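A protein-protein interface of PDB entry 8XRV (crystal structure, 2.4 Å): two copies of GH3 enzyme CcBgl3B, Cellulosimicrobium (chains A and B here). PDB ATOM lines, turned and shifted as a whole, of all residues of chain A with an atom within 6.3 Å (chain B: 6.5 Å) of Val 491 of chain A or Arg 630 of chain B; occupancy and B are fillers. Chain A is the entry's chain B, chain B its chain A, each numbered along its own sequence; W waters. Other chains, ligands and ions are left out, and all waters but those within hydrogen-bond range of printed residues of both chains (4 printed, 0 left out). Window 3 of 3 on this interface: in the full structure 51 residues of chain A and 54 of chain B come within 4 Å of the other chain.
The backbone NH of Ala 632 of chain B sits at hydrogen-bond distance from the backbone carbonyl oxygen of Ser 531 of chain A (2.6 Å).
The backbone carbonyl oxygen (O) of Ala 474 of chain A sits at hydrogen-bond distance from the backbone NH (N) of Val 491 of chain A, 2.8 Å away.
Among the printed residues, pairs that only touch across the chains: Ser 531 of chain A with Tyr 631 of chain B (3.3 Å), Val 492 of chain A with Ala 632 of chain B (3.3 Å), Gly 529 of chain A with His 627 of chain B (3.7 Å) and Val 491 of chain A with Arg 630 of chain B (3.7 Å).
Val 491 of chain A touches just one residue of chain B: Arg 630.
Of the printed residues of chain B, Val 492 of chain A touches Ala 632 (3.3 Å).
Printed residues of chain B within 4 Å of Gly 529 of chain A: His 627.
Arg 530 of chain A touches none of the printed residues of chain B.
Printed residues of chain B within 4 Å of Ser 531 of chain A: Tyr 631 and Ala 632.
Printed residues of chain A within 4 Å of His 627 of chain B: Gly 529 (3.7 Å).
Printed residues of chain A within 4 Å of Arg 630 of chain B: Val 491 (3.7 Å).
Asp 633 of chain B touches none of the printed residues of chain A.
The nearest residue of chain A that does not touch Arg 630 of chain B is Gly 529 of chain A (4.2 Å).
The nearest printed residue of chain B that does not touch Ser 531 of chain A is Asp 633 of chain B (4.4 Å).
Of the 11 printed residues of chain B, 4 touch a printed residue of chain A.
Hydrophobic or aromatic side chains of chain B within 4 Å of the printed part of chain A: Tyr 631 and Ala 632.
Along chain B the printed residues that touch a printed residue of chain A span positions 627 to 632.
Of the 12 printed residues of chain A, 4 touch a printed residue of chain B.
Among the printed residues, 5 pairs touch across the chains.
No position is printed for both chains.
Water W1 lies within hydrogen-bond range of NH1 of Arg 630 of chain B (2.6 Å), O of Ala 632 of chain B (2.8 Å), O of Val 492 of chain A (3.1 Å) and N of Leu 634 of chain B (3.5 Å).
Water W4 lies within hydrogen-bond range of the backbone carbonyl oxygen (O) of Gly 529 of chain A (2.7 Å), the backbone carbonyl oxygen (O) of Arg 630 of chain B (3.1 Å) and the backbone NH (N) of Ala 632 of chain B (3.2 Å).
Water W2 lies within hydrogen-bond range of NH1 of Arg 630 of chain B (2.8 Å), O of Ala 632 of chain B (3.0 Å) and N of Val 492 of chain A (3.0 Å).
Water W3 lies within hydrogen-bond range of the backbone NH of Ser 531 of chain A (2.9 Å), the backbone carbonyl oxygen of Gly 529 of chain A (3.1 Å) and the backbone carbonyl oxygen of Arg 630 of chain B (3.2 Å).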
ATOM      1  N   THR A 472     -19.486 -10.018  -0.182  1.00  0.00           N
ATOM      2  CA  THR A 472     -18.555 -10.243  -1.276  1.00  0.00           C
ATOM      3  C   THR A 472     -18.287 -11.742  -1.390  1.00  0.00           C
ATOM      4  O   THR A 472     -18.628 -12.533  -0.500  1.00  0.00           O
ATOM      5  CB  THR A 472     -17.249  -9.461  -1.067  1.00  0.00           C
ATOM      6  OG1 THR A 472     -16.663  -9.848   0.178  1.00  0.00           O
ATOM      7  CG2 THR A 472     -17.529  -7.973  -1.007  1.00  0.00           C
ATOM      8  N   LEU A 473     -17.676 -12.128  -2.506  1.00  0.00           N
ATOM      9  CA  LEU A 473     -17.275 -13.500  -2.775  1.00  0.00           C
ATOM     10  C   LEU A 473     -15.784 -13.680  -2.504  1.00  0.00           C
ATOM     11  O   LEU A 473     -14.996 -12.747  -2.669  1.00  0.00           O
ATOM     12  CB  LEU A 473     -17.604 -13.866  -4.218  1.00  0.00           C
ATOM     13  CG  LEU A 473     -19.113 -13.911  -4.433  1.00  0.00           C
ATOM     14  CD1 LEU A 473     -19.442 -14.275  -5.861  1.00  0.00           C
ATOM     15  CD2 LEU A 473     -19.749 -14.906  -3.467  1.00  0.00           C
ATOM     16  N   ALA A 474     -15.407 -14.882  -2.069  1.00  0.00           N
ATOM     17  CA  ALA A 474     -14.021 -15.203  -1.745  1.00  0.00           C
ATOM     18  C   ALA A 474     -13.810 -16.699  -1.926  1.00  0.00           C
ATOM     19  O   ALA A 474     -14.773 -17.459  -2.089  1.00  0.00           O
ATOM     20  CB  ALA A 474     -13.661 -14.778  -0.317  1.00  0.00           C
ATOM     21  N   PRO A 475     -12.561 -17.219  -1.953  1.00  0.00           N
ATOM     22  CA  PRO A 475     -12.396 -18.657  -1.923  1.00  0.00           C
ATOM     23  C   PRO A 475     -12.113 -19.125  -0.492  1.00  0.00           C
ATOM     24  O   PRO A 475     -11.637 -18.349   0.318  1.00  0.00           O
ATOM     25  CB  PRO A 475     -11.176 -18.880  -2.822  1.00  0.00           C
ATOM     26  CG  PRO A 475     -10.286 -17.697  -2.564  1.00  0.00           C
ATOM     27  CD  PRO A 475     -11.243 -16.569  -2.249  1.00  0.00           C
ATOM     28  N   ASP A 476     -12.502 -20.351  -0.173  1.00  0.00           N
ATOM     29  CA  ASP A 476     -12.079 -20.926   1.134  1.00  0.00           C
ATOM     30  C   ASP A 476     -10.907 -21.845   0.785  1.00  0.00           C
ATOM     31  O   ASP A 476     -10.871 -22.328  -0.368  1.00  0.00           O
ATOM     32  CB  ASP A 476     -13.227 -21.601   1.889  1.00  0.00           C
ATOM     33  CG  ASP A 476     -13.797 -22.843   1.222  1.00  0.00           C
ATOM     34  OD1 ASP A 476     -13.976 -23.851   1.931  1.00  0.00           O
ATOM     35  OD2 ASP A 476     -14.081 -22.790   0.011  1.00  0.00           O
ATOM     36  N   GLN A 490     -16.004 -17.983  -4.321  1.00  0.00           N
ATOM     37  CA  GLN A 490     -16.587 -19.283  -3.984  1.00  0.00           C
ATOM     38  C   GLN A 490     -17.634 -19.202  -2.863  1.00  0.00           C
ATOM     39  O   GLN A 490     -18.768 -19.647  -3.039  1.00  0.00           O
ATOM     40  CB  GLN A 490     -15.478 -20.272  -3.591  1.00  0.00           C
ATOM     41  CG  GLN A 490     -15.965 -21.684  -3.240  1.00  0.00           C
ATOM     42  CD  GLN A 490     -16.134 -22.555  -4.463  1.00  0.00           C
ATOM     43  OE1 GLN A 490     -16.726 -22.133  -5.459  1.00  0.00           O
ATOM     44  NE2 GLN A 490     -15.600 -23.777  -4.407  1.00  0.00           N
ATOM     45  N   VAL A 491     -17.261 -18.650  -1.712  1.00  0.00           N
ATOM     46  CA  VAL A 491     -18.168 -18.561  -0.572  1.00  0.00           C
ATOM     47  C   VAL A 491     -18.541 -17.106  -0.303  1.00  0.00           C
ATOM     48  O   VAL A 491     -17.789 -16.166  -0.598  1.00  0.00           O
ATOM     49  CB  VAL A 491     -17.583 -19.200   0.709  1.00  0.00           C
ATOM     50  CG1 VAL A 491     -17.262 -20.650   0.460  1.00  0.00           C
ATOM     51  CG2 VAL A 491     -16.349 -18.445   1.174  1.00  0.00           C
ATOM     52  N   VAL A 492     -19.720 -16.940   0.294  1.00  0.00           N
ATOM     53  CA  VAL A 492     -20.207 -15.627   0.700  1.00  0.00           C
ATOM     54  C   VAL A 492     -19.428 -15.161   1.921  1.00  0.00           C
ATOM     55  O   VAL A 492     -19.385 -15.842   2.952  1.00  0.00           O
ATOM     56  CB  VAL A 492     -21.712 -15.660   0.991  1.00  0.00           C
ATOM     57  CG1 VAL A 492     -22.132 -14.403   1.726  1.00  0.00           C
ATOM     58  CG2 VAL A 492     -22.511 -15.828  -0.302  1.00  0.00           C
ATOM     59  N   VAL A 493     -18.801 -13.996   1.801  1.00  0.00           N
ATOM     60  CA  VAL A 493     -18.265 -13.263   2.941  1.00  0.00           C
ATOM     61  C   VAL A 493     -19.232 -12.118   3.222  1.00  0.00           C
ATOM     62  O   VAL A 493     -19.342 -11.201   2.392  1.00  0.00           O
ATOM     63  CB  VAL A 493     -16.855 -12.724   2.663  1.00  0.00           C
ATOM     64  CG1 VAL A 493     -16.298 -12.115   3.917  1.00  0.00           C
ATOM     65  CG2 VAL A 493     -15.948 -13.815   2.143  1.00  0.00           C
ATOM     66  N   GLY A 529     -28.413 -25.018  -4.431  1.00  0.00           N
ATOM     67  CA  GLY A 529     -27.182 -25.042  -3.678  1.00  0.00           C
ATOM     68  C   GLY A 529     -26.997 -23.893  -2.717  1.00  0.00           C
ATOM     69  O   GLY A 529     -25.925 -23.784  -2.121  1.00  0.00           O
ATOM     70  N   ARG A 530     -27.997 -23.028  -2.538  1.00  0.00           N
ATOM     71  CA  ARG A 530     -27.832 -21.824  -1.725  1.00  0.00           C
ATOM     72  C   ARG A 530     -28.923 -21.728  -0.660  1.00  0.00           C
ATOM     73  O   ARG A 530     -29.623 -20.721  -0.517  1.00  0.00           O
ATOM     74  CB  ARG A 530     -27.778 -20.588  -2.617  1.00  0.00           C
ATOM     75  CG  ARG A 530     -26.378 -20.324  -3.153  1.00  0.00           C
ATOM     76  CD  ARG A 530     -26.389 -19.577  -4.482  1.00  0.00           C
ATOM     77  NE  ARG A 530     -27.046 -20.376  -5.507  1.00  0.00           N
ATOM     78  CZ  ARG A 530     -27.615 -19.889  -6.609  1.00  0.00           C
ATOM     79  NH1 ARG A 530     -28.201 -20.726  -7.473  1.00  0.00           N
ATOM     80  NH2 ARG A 530     -27.617 -18.571  -6.841  1.00  0.00           N
ATOM     81  N   SER A 531     -29.082 -22.802   0.107  1.00  0.00           N
ATOM     82  CA  SER A 531     -29.917 -22.734   1.293  1.00  0.00           C
ATOM     83  C   SER A 531     -29.231 -21.839   2.324  1.00  0.00           C
ATOM     84  O   SER A 531     -28.003 -21.655   2.294  1.00  0.00           O
ATOM     85  CB  SER A 531     -30.152 -24.136   1.851  1.00  0.00           C
ATOM     86  OG  SER A 531     -31.095 -24.855   1.070  1.00  0.00           O
ATOM     87  N   GLN B 626     -26.636 -34.358  -0.511  1.00  0.00           N
ATOM     88  CA  GLN B 626     -26.775 -32.907  -0.648  1.00  0.00           C
ATOM     89  C   GLN B 626     -26.075 -32.341  -1.885  1.00  0.00           C
ATOM     90  O   GLN B 626     -24.934 -32.692  -2.176  1.00  0.00           O
ATOM     91  CB  GLN B 626     -26.214 -32.231   0.593  1.00  0.00           C
ATOM     92  CG  GLN B 626     -26.452 -30.759   0.592  1.00  0.00           C
ATOM     93  CD  GLN B 626     -25.807 -30.087   1.757  1.00  0.00           C
ATOM     94  OE1 GLN B 626     -25.189 -30.740   2.606  1.00  0.00           O
ATOM     95  NE2 GLN B 626     -25.963 -28.769   1.832  1.00  0.00           N
ATOM     96  N   HIS B 627     -26.766 -31.437  -2.591  1.00  0.00           N
ATOM     97  CA  HIS B 627     -26.241 -30.560  -3.646  1.00  0.00           C
ATOM     98  C   HIS B 627     -25.560 -29.376  -2.975  1.00  0.00           C
ATOM     99  O   HIS B 627     -26.208 -28.394  -2.607  1.00  0.00           O
ATOM    100  CB  HIS B 627     -27.387 -30.056  -4.510  1.00  0.00           C
ATOM    101  CG  HIS B 627     -27.866 -31.022  -5.535  1.00  0.00           C
ATOM    102  ND1 HIS B 627     -28.199 -32.319  -5.220  1.00  0.00           N
ATOM    103  CD2 HIS B 627     -28.287 -30.827  -6.805  1.00  0.00           C
ATOM    104  CE1 HIS B 627     -28.680 -32.921  -6.291  1.00  0.00           C
ATOM    105  NE2 HIS B 627     -28.762 -32.031  -7.263  1.00  0.00           N
ATOM    106  N   GLY B 628     -24.248 -29.446  -2.812  1.00  0.00           N
ATOM    107  CA  GLY B 628     -23.506 -28.403  -2.133  1.00  0.00           C
ATOM    108  C   GLY B 628     -23.006 -28.854  -0.769  1.00  0.00           C
ATOM    109  O   GLY B 628     -23.415 -29.878  -0.217  1.00  0.00           O
ATOM    110  N   VAL B 629     -22.115 -28.041  -0.216  1.00  0.00           N
ATOM    111  CA  VAL B 629     -21.402 -28.407   0.999  1.00  0.00           C
ATOM    112  C   VAL B 629     -21.806 -27.556   2.191  1.00  0.00           C
ATOM    113  O   VAL B 629     -21.537 -27.958   3.334  1.00  0.00           O
ATOM    114  CB  VAL B 629     -19.874 -28.315   0.790  1.00  0.00           C
ATOM    115  CG1 VAL B 629     -19.465 -29.146  -0.400  1.00  0.00           C
ATOM    116  CG2 VAL B 629     -19.404 -26.849   0.663  1.00  0.00           C
ATOM    117  N   ARG B 630     -22.402 -26.386   1.973  1.00  0.00           N
ATOM    118  CA  ARG B 630     -22.563 -25.423   3.048  1.00  0.00           C
ATOM    119  C   ARG B 630     -23.848 -24.642   2.818  1.00  0.00           C
ATOM    120  O   ARG B 630     -24.386 -24.601   1.710  1.00  0.00           O
ATOM    121  CB  ARG B 630     -21.333 -24.487   3.150  1.00  0.00           C
ATOM    122  CG  ARG B 630     -21.200 -23.460   2.026  1.00  0.00           C
ATOM    123  CD  ARG B 630     -19.777 -22.887   1.906  1.00  0.00           C
ATOM    124  NE  ARG B 630     -19.217 -22.385   3.172  1.00  0.00           N
ATOM    125  CZ  ARG B 630     -19.544 -21.221   3.752  1.00  0.00           C
ATOM    126  NH1 ARG B 630     -20.443 -20.414   3.190  1.00  0.00           N
ATOM    127  NH2 ARG B 630     -18.970 -20.855   4.898  1.00  0.00           N
ATOM    128  N   TYR B 631     -24.361 -24.046   3.886  1.00  0.00           N
ATOM    129  CA  TYR B 631     -25.374 -23.025   3.693  1.00  0.00           C
ATOM    130  C   TYR B 631     -24.704 -21.793   3.117  1.00  0.00           C
ATOM    131  O   TYR B 631     -23.530 -21.524   3.379  1.00  0.00           O
ATOM    132  CB  TYR B 631     -26.076 -22.686   5.003  1.00  0.00           C
ATOM    133  CG  TYR B 631     -26.888 -23.817   5.570  1.00  0.00           C
ATOM    134  CD1 TYR B 631     -28.172 -24.073   5.104  1.00  0.00           C
ATOM    135  CD2 TYR B 631     -26.373 -24.626   6.584  1.00  0.00           C
ATOM    136  CE1 TYR B 631     -28.936 -25.111   5.629  1.00  0.00           C
ATOM    137  CE2 TYR B 631     -27.118 -25.676   7.105  1.00  0.00           C
ATOM    138  CZ  TYR B 631     -28.402 -25.912   6.627  1.00  0.00           C
ATOM    139  OH  TYR B 631     -29.153 -26.943   7.151  1.00  0.00           O
ATOM    140  N   ALA B 632     -25.444 -21.054   2.297  1.00  0.00           N
ATOM    141  CA  ALA B 632     -24.841 -19.878   1.683  1.00  0.00           C
ATOM    142  C   ALA B 632     -24.422 -18.835   2.717  1.00  0.00           C
ATOM    143  O   ALA B 632     -23.492 -18.064   2.446  1.00  0.00           O
ATOM    144  CB  ALA B 632     -25.794 -19.256   0.661  1.00  0.00           C
ATOM    145  N   ASP B 633     -25.053 -18.809   3.903  1.00  0.00           N
ATOM    146  CA  ASP B 633     -24.669 -17.875   4.962  1.00  0.00           C
ATOM    147  C   ASP B 633     -23.882 -18.523   6.096  1.00  0.00           C
ATOM    148  O   ASP B 633     -23.624 -17.853   7.104  1.00  0.00           O
ATOM    149  CB  ASP B 633     -25.889 -17.145   5.563  1.00  0.00           C
ATOM    150  CG  ASP B 633     -26.989 -18.110   6.126  1.00  0.00           C
ATOM    151  OD1 ASP B 633     -26.894 -19.351   5.938  1.00  0.00           O
ATOM    152  OD2 ASP B 633     -27.914 -17.601   6.827  1.00  0.00           O
ATOM    153  N   LEU B 634     -23.496 -19.799   5.977  1.00  0.00           N
ATOM    154  CA  LEU B 634     -22.948 -20.512   7.136  1.00  0.00           C
ATOM    155  C   LEU B 634     -22.393 -21.890   6.804  1.00  0.00           C
ATOM    156  O   LEU B 634     -23.046 -22.667   6.097  1.00  0.00           O
ATOM    157  CB  LEU B 634     -24.019 -20.679   8.220  1.00  0.00           C
ATOM    158  CG  LEU B 634     -23.487 -21.254   9.530  1.00  0.00           C
ATOM    159  CD1 LEU B 634     -22.702 -20.187  10.290  1.00  0.00           C
ATOM    160  CD2 LEU B 634     -24.637 -21.805  10.377  1.00  0.00           C
ATOM    161  N   THR B 635     -21.200 -22.206   7.321  1.00  0.00           N
ATOM    162  CA  THR B 635     -20.640 -23.549   7.193  1.00  0.00           C
ATOM    163  C   THR B 635     -21.580 -24.600   7.796  1.00  0.00           C
ATOM    164  O   THR B 635     -22.365 -24.316   8.706  1.00  0.00           O
ATOM    165  CB  THR B 635     -19.269 -23.627   7.879  1.00  0.00           C
ATOM    166  OG1 THR B 635     -18.679 -24.909   7.626  1.00  0.00           O
ATOM    167  CG2 THR B 635     -19.374 -23.399   9.406  1.00  0.00           C
ATOM    168  N   GLN B 636     -21.499 -25.829   7.272  1.00  0.00           N
ATOM    169  CA  GLN B 636     -22.160 -26.971   7.889  1.00  0.00           C
ATOM    170  C   GLN B 636     -21.259 -27.686   8.881  1.00  0.00           C
ATOM    171  O   GLN B 636     -21.701 -28.623   9.552  1.00  0.00           O
ATOM    172  CB  GLN B 636     -22.665 -27.933   6.822  1.00  0.00           C
ATOM    173  CG  GLN B 636     -23.719 -27.256   5.976  1.00  0.00           C
ATOM    174  CD  GLN B 636     -24.400 -28.143   4.970  1.00  0.00           C
ATOM    175  OE1 GLN B 636     -25.154 -27.650   4.126  1.00  0.00           O
ATOM    176  NE2 GLN B 636     -24.155 -29.446   5.040  1.00  0.00           N
HETATM  177  O   HOH W   1     -21.214 -18.043   4.034  1.00  0.00           O
HETATM  178  O   HOH W   2     -21.392 -19.408   0.812  1.00  0.00           O
HETATM  179  O   HOH W   3     -27.220 -25.058   0.352  1.00  0.00           O
HETATM  180  O   HOH W   4     -24.342 -22.334  -0.435  1.00  0.00           O
